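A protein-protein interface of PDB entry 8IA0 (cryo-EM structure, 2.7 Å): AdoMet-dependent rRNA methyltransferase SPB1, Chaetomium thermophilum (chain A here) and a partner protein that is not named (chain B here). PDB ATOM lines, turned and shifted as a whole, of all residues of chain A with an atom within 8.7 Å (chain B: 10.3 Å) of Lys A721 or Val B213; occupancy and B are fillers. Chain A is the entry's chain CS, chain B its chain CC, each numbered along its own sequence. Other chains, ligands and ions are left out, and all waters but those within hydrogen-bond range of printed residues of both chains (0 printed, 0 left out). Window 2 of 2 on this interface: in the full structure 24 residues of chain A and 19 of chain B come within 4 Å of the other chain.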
ATOM      1  N   ASN A 651       0.880   3.773  -1.230  1.00  0.00           N
ATOM      2  CA  ASN A 651       0.572   2.485  -1.831  1.00  0.00           C
ATOM      3  C   ASN A 651      -0.760   1.968  -1.308  1.00  0.00           C
ATOM      4  O   ASN A 651      -1.023   1.982  -0.102  1.00  0.00           O
ATOM      5  CB  ASN A 651       1.679   1.470  -1.552  1.00  0.00           C
ATOM      6  CG  ASN A 651       2.194   1.542  -0.132  1.00  0.00           C
ATOM      7  OD1 ASN A 651       2.413   2.624   0.404  1.00  0.00           O
ATOM      8  ND2 ASN A 651       2.391   0.384   0.486  1.00  0.00           N
ATOM      9  N   ILE A 652      -1.602   1.506  -2.224  1.00  0.00           N
ATOM     10  CA  ILE A 652      -2.929   0.997  -1.899  1.00  0.00           C
ATOM     11  C   ILE A 652      -2.830  -0.518  -1.852  1.00  0.00           C
ATOM     12  O   ILE A 652      -2.568  -1.166  -2.872  1.00  0.00           O
ATOM     13  CB  ILE A 652      -3.982   1.455  -2.916  1.00  0.00           C
ATOM     14  CG1 ILE A 652      -3.950   2.976  -3.062  1.00  0.00           C
ATOM     15  CG2 ILE A 652      -5.361   0.984  -2.497  1.00  0.00           C
ATOM     16  CD1 ILE A 652      -5.040   3.525  -3.951  1.00  0.00           C
ATOM     17  N   ASP A 653      -3.046  -1.087  -0.670  1.00  0.00           N
ATOM     18  CA  ASP A 653      -2.870  -2.513  -0.440  1.00  0.00           C
ATOM     19  C   ASP A 653      -4.215  -3.124  -0.078  1.00  0.00           C
ATOM     20  O   ASP A 653      -4.802  -2.776   0.951  1.00  0.00           O
ATOM     21  CB  ASP A 653      -1.827  -2.756   0.653  1.00  0.00           C
ATOM     22  CG  ASP A 653      -1.996  -4.089   1.339  1.00  0.00           C
ATOM     23  OD1 ASP A 653      -1.576  -5.117   0.768  1.00  0.00           O
ATOM     24  OD2 ASP A 653      -2.525  -4.099   2.467  1.00  0.00           O
ATOM     25  N   ILE A 654      -4.696  -4.029  -0.924  1.00  0.00           N
ATOM     26  CA  ILE A 654      -6.026  -4.610  -0.772  1.00  0.00           C
ATOM     27  C   ILE A 654      -5.946  -5.800   0.175  1.00  0.00           C
ATOM     28  O   ILE A 654      -5.259  -6.787  -0.108  1.00  0.00           O
ATOM     29  CB  ILE A 654      -6.605  -5.024  -2.131  1.00  0.00           C
ATOM     30  CG1 ILE A 654      -6.803  -3.795  -3.019  1.00  0.00           C
ATOM     31  CG2 ILE A 654      -7.915  -5.763  -1.950  1.00  0.00           C
ATOM     32  CD1 ILE A 654      -6.972  -4.120  -4.482  1.00  0.00           C
ATOM     33  N   ILE A 655      -6.652  -5.706   1.302  1.00  0.00           N
ATOM     34  CA  ILE A 655      -6.704  -6.778   2.287  1.00  0.00           C
ATOM     35  C   ILE A 655      -8.124  -7.204   2.615  1.00  0.00           C
ATOM     36  O   ILE A 655      -8.315  -8.064   3.476  1.00  0.00           O
ATOM     37  CB  ILE A 655      -5.963  -6.387   3.581  1.00  0.00           C
ATOM     38  CG1 ILE A 655      -6.543  -5.092   4.153  1.00  0.00           C
ATOM     39  CG2 ILE A 655      -4.475  -6.280   3.334  1.00  0.00           C
ATOM     40  CD1 ILE A 655      -5.666  -4.430   5.189  1.00  0.00           C
ATOM     41  N   THR A 656      -9.126  -6.634   1.959  1.00  0.00           N
ATOM     42  CA  THR A 656     -10.519  -6.841   2.314  1.00  0.00           C
ATOM     43  C   THR A 656     -11.211  -7.651   1.227  1.00  0.00           C
ATOM     44  O   THR A 656     -10.951  -7.457   0.035  1.00  0.00           O
ATOM     45  CB  THR A 656     -11.226  -5.498   2.512  1.00  0.00           C
ATOM     46  OG1 THR A 656     -10.377  -4.624   3.266  1.00  0.00           O
ATOM     47  CG2 THR A 656     -12.507  -5.686   3.283  1.00  0.00           C
ATOM     48  N   ALA A 659     -13.211  -5.571  -1.195  1.00  0.00           N
ATOM     49  CA  ALA A 659     -12.310  -4.815  -2.060  1.00  0.00           C
ATOM     50  C   ALA A 659     -11.733  -5.698  -3.159  1.00  0.00           C
ATOM     51  O   ALA A 659     -11.613  -5.269  -4.312  1.00  0.00           O
ATOM     52  CB  ALA A 659     -11.192  -4.185  -1.233  1.00  0.00           C
ATOM     53  N   MET A 660     -11.365  -6.935  -2.818  1.00  0.00           N
ATOM     54  CA  MET A 660     -10.855  -7.863  -3.821  1.00  0.00           C
ATOM     55  C   MET A 660     -11.925  -8.185  -4.856  1.00  0.00           C
ATOM     56  O   MET A 660     -11.622  -8.365  -6.040  1.00  0.00           O
ATOM     57  CB  MET A 660     -10.365  -9.143  -3.146  1.00  0.00           C
ATOM     58  CG  MET A 660      -9.329  -9.949  -3.927  1.00  0.00           C
ATOM     59  SD  MET A 660      -7.830  -9.030  -4.341  1.00  0.00           S
ATOM     60  CE  MET A 660      -8.133  -8.564  -6.038  1.00  0.00           C
ATOM     61  N   ALA A 714     -12.482 -14.137  -4.788  1.00  0.00           N
ATOM     62  CA  ALA A 714     -11.969 -13.003  -4.027  1.00  0.00           C
ATOM     63  C   ALA A 714     -11.566 -13.422  -2.619  1.00  0.00           C
ATOM     64  O   ALA A 714     -10.541 -12.968  -2.098  1.00  0.00           O
ATOM     65  CB  ALA A 714     -13.009 -11.886  -3.980  1.00  0.00           C
ATOM     66  N   ALA A 715     -12.366 -14.282  -1.986  1.00  0.00           N
ATOM     67  CA  ALA A 715     -12.041 -14.745  -0.642  1.00  0.00           C
ATOM     68  C   ALA A 715     -10.762 -15.571  -0.635  1.00  0.00           C
ATOM     69  O   ALA A 715      -9.938 -15.445   0.278  1.00  0.00           O
ATOM     70  CB  ALA A 715     -13.204 -15.553  -0.069  1.00  0.00           C
ATOM     71  N   GLN A 716     -10.581 -16.428  -1.642  1.00  0.00           N
ATOM     72  CA  GLN A 716      -9.379 -17.253  -1.704  1.00  0.00           C
ATOM     73  C   GLN A 716      -8.131 -16.401  -1.895  1.00  0.00           C
ATOM     74  O   GLN A 716      -7.087 -16.673  -1.293  1.00  0.00           O
ATOM     75  CB  GLN A 716      -9.502 -18.280  -2.831  1.00  0.00           C
ATOM     76  CG  GLN A 716      -9.907 -19.692  -2.399  1.00  0.00           C
ATOM     77  CD  GLN A 716      -9.049 -20.270  -1.280  1.00  0.00           C
ATOM     78  OE1 GLN A 716      -9.097 -19.821  -0.135  1.00  0.00           O
ATOM     79  NE2 GLN A 716      -8.256 -21.281  -1.616  1.00  0.00           N
ATOM     80  N   ALA A 717      -8.216 -15.372  -2.740  1.00  0.00           N
ATOM     81  CA  ALA A 717      -7.056 -14.525  -2.990  1.00  0.00           C
ATOM     82  C   ALA A 717      -6.619 -13.799  -1.726  1.00  0.00           C
ATOM     83  O   ALA A 717      -5.418 -13.658  -1.466  1.00  0.00           O
ATOM     84  CB  ALA A 717      -7.362 -13.527  -4.105  1.00  0.00           C
ATOM     85  N   ILE A 718      -7.579 -13.323  -0.932  1.00  0.00           N
ATOM     86  CA  ILE A 718      -7.243 -12.653   0.320  1.00  0.00           C
ATOM     87  C   ILE A 718      -6.565 -13.623   1.278  1.00  0.00           C
ATOM     88  O   ILE A 718      -5.586 -13.273   1.949  1.00  0.00           O
ATOM     89  CB  ILE A 718      -8.504 -12.022   0.941  1.00  0.00           C
ATOM     90  CG1 ILE A 718      -8.973 -10.846   0.088  1.00  0.00           C
ATOM     91  CG2 ILE A 718      -8.235 -11.566   2.361  1.00  0.00           C
ATOM     92  CD1 ILE A 718      -7.925  -9.777  -0.097  1.00  0.00           C
ATOM     93  N   LYS A 719      -7.069 -14.856   1.354  1.00  0.00           N
ATOM     94  CA  LYS A 719      -6.433 -15.862   2.197  1.00  0.00           C
ATOM     95  C   LYS A 719      -5.017 -16.163   1.722  1.00  0.00           C
ATOM     96  O   LYS A 719      -4.101 -16.322   2.535  1.00  0.00           O
ATOM     97  CB  LYS A 719      -7.276 -17.136   2.217  1.00  0.00           C
ATOM     98  CG  LYS A 719      -8.332 -17.160   3.306  1.00  0.00           C
ATOM     99  CD  LYS A 719      -9.092 -18.475   3.310  1.00  0.00           C
ATOM    100  CE  LYS A 719     -10.557 -18.265   2.966  1.00  0.00           C
ATOM    101  NZ  LYS A 719     -11.090 -19.360   2.109  1.00  0.00           N
ATOM    102  N   GLU A 720      -4.820 -16.248   0.404  1.00  0.00           N
ATOM    103  CA  GLU A 720      -3.482 -16.468  -0.130  1.00  0.00           C
ATOM    104  C   GLU A 720      -2.590 -15.254   0.092  1.00  0.00           C
ATOM    105  O   GLU A 720      -1.401 -15.398   0.398  1.00  0.00           O
ATOM    106  CB  GLU A 720      -3.562 -16.811  -1.618  1.00  0.00           C
ATOM    107  CG  GLU A 720      -2.263 -17.326  -2.207  1.00  0.00           C
ATOM    108  CD  GLU A 720      -2.411 -17.759  -3.652  1.00  0.00           C
ATOM    109  OE1 GLU A 720      -3.553 -17.760  -4.159  1.00  0.00           O
ATOM    110  OE2 GLU A 720      -1.387 -18.099  -4.280  1.00  0.00           O
ATOM    111  N   LYS A 721      -3.145 -14.051  -0.060  1.00  0.00           N
ATOM    112  CA  LYS A 721      -2.344 -12.838   0.077  1.00  0.00           C
ATOM    113  C   LYS A 721      -1.896 -12.621   1.518  1.00  0.00           C
ATOM    114  O   LYS A 721      -0.768 -12.177   1.762  1.00  0.00           O
ATOM    115  CB  LYS A 721      -3.136 -11.634  -0.427  1.00  0.00           C
ATOM    116  CG  LYS A 721      -2.337 -10.350  -0.495  1.00  0.00           C
ATOM    117  CD  LYS A 721      -3.172  -9.216  -1.056  1.00  0.00           C
ATOM    118  CE  LYS A 721      -2.374  -7.926  -1.112  1.00  0.00           C
ATOM    119  NZ  LYS A 721      -3.165  -6.813  -1.702  1.00  0.00           N
ATOM    120  N   LEU A 722      -2.759 -12.927   2.483  1.00  0.00           N
ATOM    121  CA  LEU A 722      -2.451 -12.722   3.892  1.00  0.00           C
ATOM    122  C   LEU A 722      -1.815 -13.939   4.547  1.00  0.00           C
ATOM    123  O   LEU A 722      -1.563 -13.912   5.756  1.00  0.00           O
ATOM    124  CB  LEU A 722      -3.718 -12.335   4.659  1.00  0.00           C
ATOM    125  CG  LEU A 722      -4.436 -11.072   4.185  1.00  0.00           C
ATOM    126  CD1 LEU A 722      -5.611 -10.754   5.091  1.00  0.00           C
ATOM    127  CD2 LEU A 722      -3.470  -9.904   4.124  1.00  0.00           C
ATOM    128  N   ARG A 723      -1.559 -15.000   3.789  1.00  0.00           N
ATOM    129  CA  ARG A 723      -0.897 -16.174   4.337  1.00  0.00           C
ATOM    130  C   ARG A 723       0.532 -15.835   4.739  1.00  0.00           C
ATOM    131  O   ARG A 723       1.250 -15.150   4.006  1.00  0.00           O
ATOM    132  CB  ARG A 723      -0.917 -17.302   3.306  1.00  0.00           C
ATOM    133  CG  ARG A 723      -0.209 -18.575   3.721  1.00  0.00           C
ATOM    134  CD  ARG A 723      -0.855 -19.780   3.056  1.00  0.00           C
ATOM    135  NE  ARG A 723       0.106 -20.791   2.633  1.00  0.00           N
ATOM    136  CZ  ARG A 723       1.018 -20.621   1.685  1.00  0.00           C
ATOM    137  NH1 ARG A 723       1.114 -19.488   1.009  1.00  0.00           N
ATOM    138  NH2 ARG A 723       1.850 -21.619   1.399  1.00  0.00           N
ATOM    139  N   ALA A 724       0.940 -16.313   5.909  1.00  0.00           N
ATOM    140  CA  ALA A 724       2.274 -16.036   6.412  1.00  0.00           C
ATOM    141  C   ALA A 724       3.302 -16.927   5.719  1.00  0.00           C
ATOM    142  O   ALA A 724       2.971 -17.922   5.072  1.00  0.00           O
ATOM    143  CB  ALA A 724       2.328 -16.232   7.925  1.00  0.00           C
ATOM    144  N   LEU A 725       4.573 -16.554   5.866  1.00  0.00           N
ATOM    145  CA  LEU A 725       5.650 -17.314   5.248  1.00  0.00           C
ATOM    146  C   LEU A 725       6.000 -18.576   6.023  1.00  0.00           C
ATOM    147  O   LEU A 725       6.698 -19.441   5.485  1.00  0.00           O
ATOM    148  CB  LEU A 725       6.897 -16.441   5.104  1.00  0.00           C
ATOM    149  CG  LEU A 725       7.887 -16.842   4.009  1.00  0.00           C
ATOM    150  CD1 LEU A 725       7.166 -17.044   2.692  1.00  0.00           C
ATOM    151  CD2 LEU A 725       8.981 -15.803   3.867  1.00  0.00           C
ATOM    152  N   GLN B 205      11.934 -14.411 -10.061  1.00  0.00           N
ATOM    153  CA  GLN B 205      10.927 -13.357 -10.013  1.00  0.00           C
ATOM    154  C   GLN B 205       9.615 -13.876  -9.442  1.00  0.00           C
ATOM    155  O   GLN B 205       8.924 -13.162  -8.707  1.00  0.00           O
ATOM    156  CB  GLN B 205      10.716 -12.770 -11.407  1.00  0.00           C
ATOM    157  CG  GLN B 205       9.764 -11.588 -11.443  1.00  0.00           C
ATOM    158  CD  GLN B 205      10.239 -10.433 -10.586  1.00  0.00           C
ATOM    159  OE1 GLN B 205      11.406 -10.046 -10.639  1.00  0.00           O
ATOM    160  NE2 GLN B 205       9.335  -9.874  -9.792  1.00  0.00           N
ATOM    161  N   ASN B 206       9.253 -15.117  -9.776  1.00  0.00           N
ATOM    162  CA  ASN B 206       8.045 -15.709  -9.212  1.00  0.00           C
ATOM    163  C   ASN B 206       8.157 -15.856  -7.701  1.00  0.00           C
ATOM    164  O   ASN B 206       7.190 -15.605  -6.972  1.00  0.00           O
ATOM    165  CB  ASN B 206       7.771 -17.065  -9.861  1.00  0.00           C
ATOM    166  CG  ASN B 206       6.998 -16.944 -11.154  1.00  0.00           C
ATOM    167  OD1 ASN B 206       7.580 -16.778 -12.225  1.00  0.00           O
ATOM    168  ND2 ASN B 206       5.677 -17.027 -11.063  1.00  0.00           N
ATOM    169  N   LEU B 207       9.328 -16.267  -7.212  1.00  0.00           N
ATOM    170  CA  LEU B 207       9.524 -16.392  -5.773  1.00  0.00           C
ATOM    171  C   LEU B 207       9.438 -15.035  -5.087  1.00  0.00           C
ATOM    172  O   LEU B 207       8.882 -14.921  -3.988  1.00  0.00           O
ATOM    173  CB  LEU B 207      10.868 -17.058  -5.484  1.00  0.00           C
ATOM    174  CG  LEU B 207      10.849 -18.584  -5.394  1.00  0.00           C
ATOM    175  CD1 LEU B 207      12.248 -19.142  -5.564  1.00  0.00           C
ATOM    176  CD2 LEU B 207      10.245 -19.037  -4.078  1.00  0.00           C
ATOM    177  N   LEU B 208       9.991 -13.997  -5.715  1.00  0.00           N
ATOM    178  CA  LEU B 208       9.886 -12.655  -5.156  1.00  0.00           C
ATOM    179  C   LEU B 208       8.438 -12.192  -5.101  1.00  0.00           C
ATOM    180  O   LEU B 208       8.009 -11.591  -4.111  1.00  0.00           O
ATOM    181  CB  LEU B 208      10.725 -11.678  -5.978  1.00  0.00           C
ATOM    182  CG  LEU B 208      12.087 -11.309  -5.396  1.00  0.00           C
ATOM    183  CD1 LEU B 208      12.785 -10.297  -6.286  1.00  0.00           C
ATOM    184  CD2 LEU B 208      11.931 -10.772  -3.985  1.00  0.00           C
ATOM    185  N   ASP B 209       7.670 -12.463  -6.158  1.00  0.00           N
ATOM    186  CA  ASP B 209       6.266 -12.064  -6.170  1.00  0.00           C
ATOM    187  C   ASP B 209       5.476 -12.803  -5.099  1.00  0.00           C
ATOM    188  O   ASP B 209       4.576 -12.230  -4.474  1.00  0.00           O
ATOM    189  CB  ASP B 209       5.663 -12.310  -7.551  1.00  0.00           C
ATOM    190  CG  ASP B 209       6.303 -11.454  -8.625  1.00  0.00           C
ATOM    191  OD1 ASP B 209       7.265 -10.722  -8.310  1.00  0.00           O
ATOM    192  OD2 ASP B 209       5.843 -11.510  -9.786  1.00  0.00           O
ATOM    193  N   SER B 210       5.792 -14.081  -4.879  1.00  0.00           N
ATOM    194  CA  SER B 210       5.099 -14.845  -3.848  1.00  0.00           C
ATOM    195  C   SER B 210       5.399 -14.301  -2.456  1.00  0.00           C
ATOM    196  O   SER B 210       4.501 -14.208  -1.613  1.00  0.00           O
ATOM    197  CB  SER B 210       5.484 -16.320  -3.943  1.00  0.00           C
ATOM    198  OG  SER B 210       6.854 -16.508  -3.633  1.00  0.00           O
ATOM    199  N   ILE B 211       6.656 -13.941  -2.197  1.00  0.00           N
ATOM    200  CA  ILE B 211       7.037 -13.461  -0.872  1.00  0.00           C
ATOM    201  C   ILE B 211       6.431 -12.090  -0.602  1.00  0.00           C
ATOM    202  O   ILE B 211       5.834 -11.853   0.454  1.00  0.00           O
ATOM    203  CB  ILE B 211       8.569 -13.441  -0.733  1.00  0.00           C
ATOM    204  CG1 ILE B 211       9.084 -14.845  -0.434  1.00  0.00           C
ATOM    205  CG2 ILE B 211       8.997 -12.478   0.356  1.00  0.00           C
ATOM    206  CD1 ILE B 211      10.565 -14.904  -0.249  1.00  0.00           C
ATOM    207  N   GLU B 212       6.571 -11.169  -1.549  1.00  0.00           N
ATOM    208  CA  GLU B 212       6.003  -9.827  -1.447  1.00  0.00           C
ATOM    209  C   GLU B 212       5.074  -9.635  -2.642  1.00  0.00           C
ATOM    210  O   GLU B 212       5.522  -9.435  -3.773  1.00  0.00           O
ATOM    211  CB  GLU B 212       7.099  -8.754  -1.376  1.00  0.00           C
ATOM    212  CG  GLU B 212       8.208  -8.892  -2.407  1.00  0.00           C
ATOM    213  CD  GLU B 212       9.046  -7.636  -2.531  1.00  0.00           C
ATOM    214  OE1 GLU B 212       9.646  -7.219  -1.519  1.00  0.00           O
ATOM    215  OE2 GLU B 212       9.106  -7.067  -3.641  1.00  0.00           O
ATOM    216  N   VAL B 213       3.773  -9.716  -2.383  1.00  0.00           N
ATOM    217  CA  VAL B 213       2.796  -9.650  -3.473  1.00  0.00           C
ATOM    218  C   VAL B 213       2.844  -8.270  -4.110  1.00  0.00           C
ATOM    219  O   VAL B 213       2.986  -7.260  -3.390  1.00  0.00           O
ATOM    220  CB  VAL B 213       1.384  -9.970  -2.957  1.00  0.00           C
ATOM    221  CG1 VAL B 213       1.200 -11.469  -2.821  1.00  0.00           C
ATOM    222  CG2 VAL B 213       1.141  -9.281  -1.625  1.00  0.00           C
ATOM    223  N   PRO B 214       2.749  -8.156  -5.432  1.00  0.00           N
ATOM    224  CA  PRO B 214       2.705  -6.831  -6.055  1.00  0.00           C
ATOM    225  C   PRO B 214       1.446  -6.080  -5.652  1.00  0.00           C
ATOM    226  O   PRO B 214       0.472  -6.656  -5.163  1.00  0.00           O
ATOM    227  CB  PRO B 214       2.716  -7.141  -7.558  1.00  0.00           C
ATOM    228  CG  PRO B 214       3.282  -8.516  -7.658  1.00  0.00           C
ATOM    229  CD  PRO B 214       2.810  -9.232  -6.433  1.00  0.00           C
ATOM    230  N   GLU B 215       1.483  -4.763  -5.860  1.00  0.00           N
ATOM    231  CA  GLU B 215       0.372  -3.919  -5.439  1.00  0.00           C
ATOM    232  C   GLU B 215      -0.912  -4.278  -6.176  1.00  0.00           C
ATOM    233  O   GLU B 215      -1.992  -4.310  -5.576  1.00  0.00           O
ATOM    234  CB  GLU B 215       0.724  -2.448  -5.657  1.00  0.00           C
ATOM    235  CG  GLU B 215       0.080  -1.504  -4.662  1.00  0.00           C
ATOM    236  CD  GLU B 215      -0.028  -0.088  -5.192  1.00  0.00           C
ATOM    237  OE1 GLU B 215       0.225   0.117  -6.397  1.00  0.00           O
ATOM    238  OE2 GLU B 215      -0.375   0.817  -4.405  1.00  0.00           O
ATOM    239  N   GLY B 216      -0.816  -4.556  -7.473  1.00  0.00           N
ATOM    240  CA  GLY B 216      -1.995  -4.837  -8.267  1.00  0.00           C
ATOM    241  C   GLY B 216      -2.333  -6.309  -8.378  1.00  0.00           C
ATOM    242  O   GLY B 216      -3.110  -6.704  -9.251  1.00  0.00           O
ATOM    243  N   TRP B 217      -1.759  -7.128  -7.501  1.00  0.00           N
ATOM    244  CA  TRP B 217      -1.982  -8.566  -7.559  1.00  0.00           C
ATOM    245  C   TRP B 217      -3.450  -8.895  -7.315  1.00  0.00           C
ATOM    246  O   TRP B 217      -4.063  -8.395  -6.370  1.00  0.00           O
ATOM    247  CB  TRP B 217      -1.102  -9.271  -6.528  1.00  0.00           C
ATOM    248  CG  TRP B 217      -1.148 -10.764  -6.604  1.00  0.00           C
ATOM    249  CD1 TRP B 217      -0.454 -11.561  -7.463  1.00  0.00           C
ATOM    250  CD2 TRP B 217      -1.919 -11.642  -5.777  1.00  0.00           C
ATOM    251  NE1 TRP B 217      -0.750 -12.880  -7.231  1.00  0.00           N
ATOM    252  CE2 TRP B 217      -1.646 -12.957  -6.199  1.00  0.00           C
ATOM    253  CE3 TRP B 217      -2.816 -11.445  -4.726  1.00  0.00           C
ATOM    254  CZ2 TRP B 217      -2.238 -14.067  -5.606  1.00  0.00           C
ATOM    255  CZ3 TRP B 217      -3.403 -12.548  -4.139  1.00  0.00           C
ATOM    256  CH2 TRP B 217      -3.112 -13.842  -4.580  1.00  0.00           C
ATOM    257  N   THR B 218      -4.012  -9.740  -8.180  1.00  0.00           N
ATOM    258  CA  THR B 218      -5.403 -10.161  -8.063  1.00  0.00           C
ATOM    259  C   THR B 218      -5.598 -11.666  -8.014  1.00  0.00           C
ATOM    260  O   THR B 218      -6.674 -12.108  -7.598  1.00  0.00           O
ATOM    261  CB  THR B 218      -6.238  -9.607  -9.227  1.00  0.00           C
ATOM    262  OG1 THR B 218      -5.694 -10.073 -10.469  1.00  0.00           O
ATOM    263  CG2 THR B 218      -6.229  -8.095  -9.218  1.00  0.00           C
ATOM    264  N   GLY B 219      -4.614 -12.463  -8.417  1.00  0.00           N
ATOM    265  CA  GLY B 219      -4.786 -13.898  -8.470  1.00  0.00           C
ATOM    266  C   GLY B 219      -5.474 -14.408  -9.713  1.00  0.00           C
ATOM    267  O   GLY B 219      -5.709 -15.616  -9.820  1.00  0.00           O
ATOM    268  N   ASN B 230      -2.667  -7.865 -13.455  1.00  0.00           N
ATOM    269  CA  ASN B 230      -2.351  -6.938 -12.381  1.00  0.00           C
ATOM    270  C   ASN B 230      -3.065  -5.615 -12.617  1.00  0.00           C
ATOM    271  O   ASN B 230      -3.102  -5.111 -13.743  1.00  0.00           O
ATOM    272  CB  ASN B 230      -0.842  -6.707 -12.276  1.00  0.00           C
ATOM    273  CG  ASN B 230      -0.148  -7.769 -11.451  1.00  0.00           C
ATOM    274  OD1 ASN B 230      -0.704  -8.838 -11.202  1.00  0.00           O
ATOM    275  ND2 ASN B 230       1.076  -7.481 -11.023  1.00  0.00           N
ATOM    276  N   LEU B 231      -3.632  -5.061 -11.550  1.00  0.00           N
ATOM    277  CA  LEU B 231      -4.240  -3.745 -11.633  1.00  0.00           C
ATOM    278  C   LEU B 231      -3.163  -2.674 -11.769  1.00  0.00           C
ATOM    279  O   LEU B 231      -2.002  -2.867 -11.402  1.00  0.00           O
ATOM    280  CB  LEU B 231      -5.092  -3.463 -10.398  1.00  0.00           C
ATOM    281  CG  LEU B 231      -6.335  -4.319 -10.166  1.00  0.00           C
ATOM    282  CD1 LEU B 231      -6.486  -4.596  -8.682  1.00  0.00           C
ATOM    283  CD2 LEU B 231      -7.570  -3.635 -10.711  1.00  0.00           C
ATOM    284  N   LEU B 236      -6.335   1.157  -9.043  1.00  0.00           N
ATOM    285  CA  LEU B 236      -6.294   1.016  -7.590  1.00  0.00           C
ATOM    286  C   LEU B 236      -6.883   2.238  -6.899  1.00  0.00           C
ATOM    287  O   LEU B 236      -7.532   2.117  -5.854  1.00  0.00           O
ATOM    288  CB  LEU B 236      -4.858   0.780  -7.122  1.00  0.00           C
ATOM    289  CG  LEU B 236      -4.267  -0.599  -7.412  1.00  0.00           C
ATOM    290  CD1 LEU B 236      -2.758  -0.511  -7.522  1.00  0.00           C
ATOM    291  CD2 LEU B 236      -4.668  -1.591  -6.335  1.00  0.00           C
ATOM    292  N   ILE B 239     -10.741   1.832  -6.985  1.00  0.00           N
ATOM    293  CA  ILE B 239     -11.242   0.961  -5.923  1.00  0.00           C
ATOM    294  C   ILE B 239     -11.174   1.670  -4.577  1.00  0.00           C
ATOM    295  O   ILE B 239     -12.092   1.561  -3.756  1.00  0.00           O
ATOM    296  CB  ILE B 239     -10.478  -0.379  -5.899  1.00  0.00           C
ATOM    297  CG1 ILE B 239     -10.959  -1.311  -7.013  1.00  0.00           C
ATOM    298  CG2 ILE B 239     -10.626  -1.067  -4.551  1.00  0.00           C
ATOM    299  CD1 ILE B 239     -10.231  -1.169  -8.310  1.00  0.00           C
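N of Ile A652 lies within hydrogen-bond range of OE2 of Glu B215.
The side-chain carboxylate (OD1) of Asp A653 is in salt-bridge range of the side-chain amino group (NZ) of Lys A721 (3.4 Å).
The side-chain amino group of Lys A721 is in hydrogen-bond range of the backbone carbonyl oxygen of Ile A654, at 2.6 Å.
OE2 of Glu B215 touches CA of Asn A651, at 3.2 Å.
O of Leu B236 touches CD1 of Ile A652, 3.4 Å away.
CD2 of Leu B236 touches CD1 of Ile A654, at 3.9 Å.
Met A660 touches Thr B218.
O of Ala A717 touches CZ3 of Trp B217 (3.5 Å).
Thr B218 touches Ala A717 (O to CB, 3.8 Å).
Glu A720 touches Trp B217 (OE1 to CH2, 3.97 Å).
Lys A721 touches Val B213 (CE to CG2, 3.8 Å).
Trp B217 touches Lys A721 (CZ3 to CB, 3.8 Å).
Of the printed residues of chain B, Ile A652 touches Glu B215 and Leu B236.
No residue of chain B comes within 4 Å of Asp A653.
Ile A654 touches just one residue of chain B: Leu B236.
Glu A720 touches just one residue of chain B: Trp B217 (3.97 Å).
Lys A721 touches two residues of chain B.
No residue of chain B comes within 4 Å of Leu A722.
Of chain A, only Lys A721 comes within 4 Å of Val B213.
No residue of chain A comes within 4 Å of Pro B214.
Printed residues of chain A within 4 Å of Glu B215: Asn A651 (3.2 Å) and Ile A652 (2.6 Å).
Leu B231 touches none of the printed residues of chain A.
Printed residues of chain A within 4 Å of Leu B236: Ile A652 (3.4 Å) and Ile A654 (3.9 Å).
Printed residues of chain B that touch a printed residue of chain A: Val B213, Glu B215, Trp B217, Thr B218 and Leu B236.
Hydrophobic or aromatic side chains of chain B within 4 Å of the printed part of chain A: Val B213, Trp B217 and Leu B236.
Along chain B the printed residues that touch a printed residue of chain A span positions 213 to 236.
Hydrophobic or aromatic side chains of chain A within 4 Å of the printed part of chain B: Ile A652, Ile A654, Met A660 and Ala A717.
Along chain A the printed residues that touch a printed residue of chain B span positions 651 to 721.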
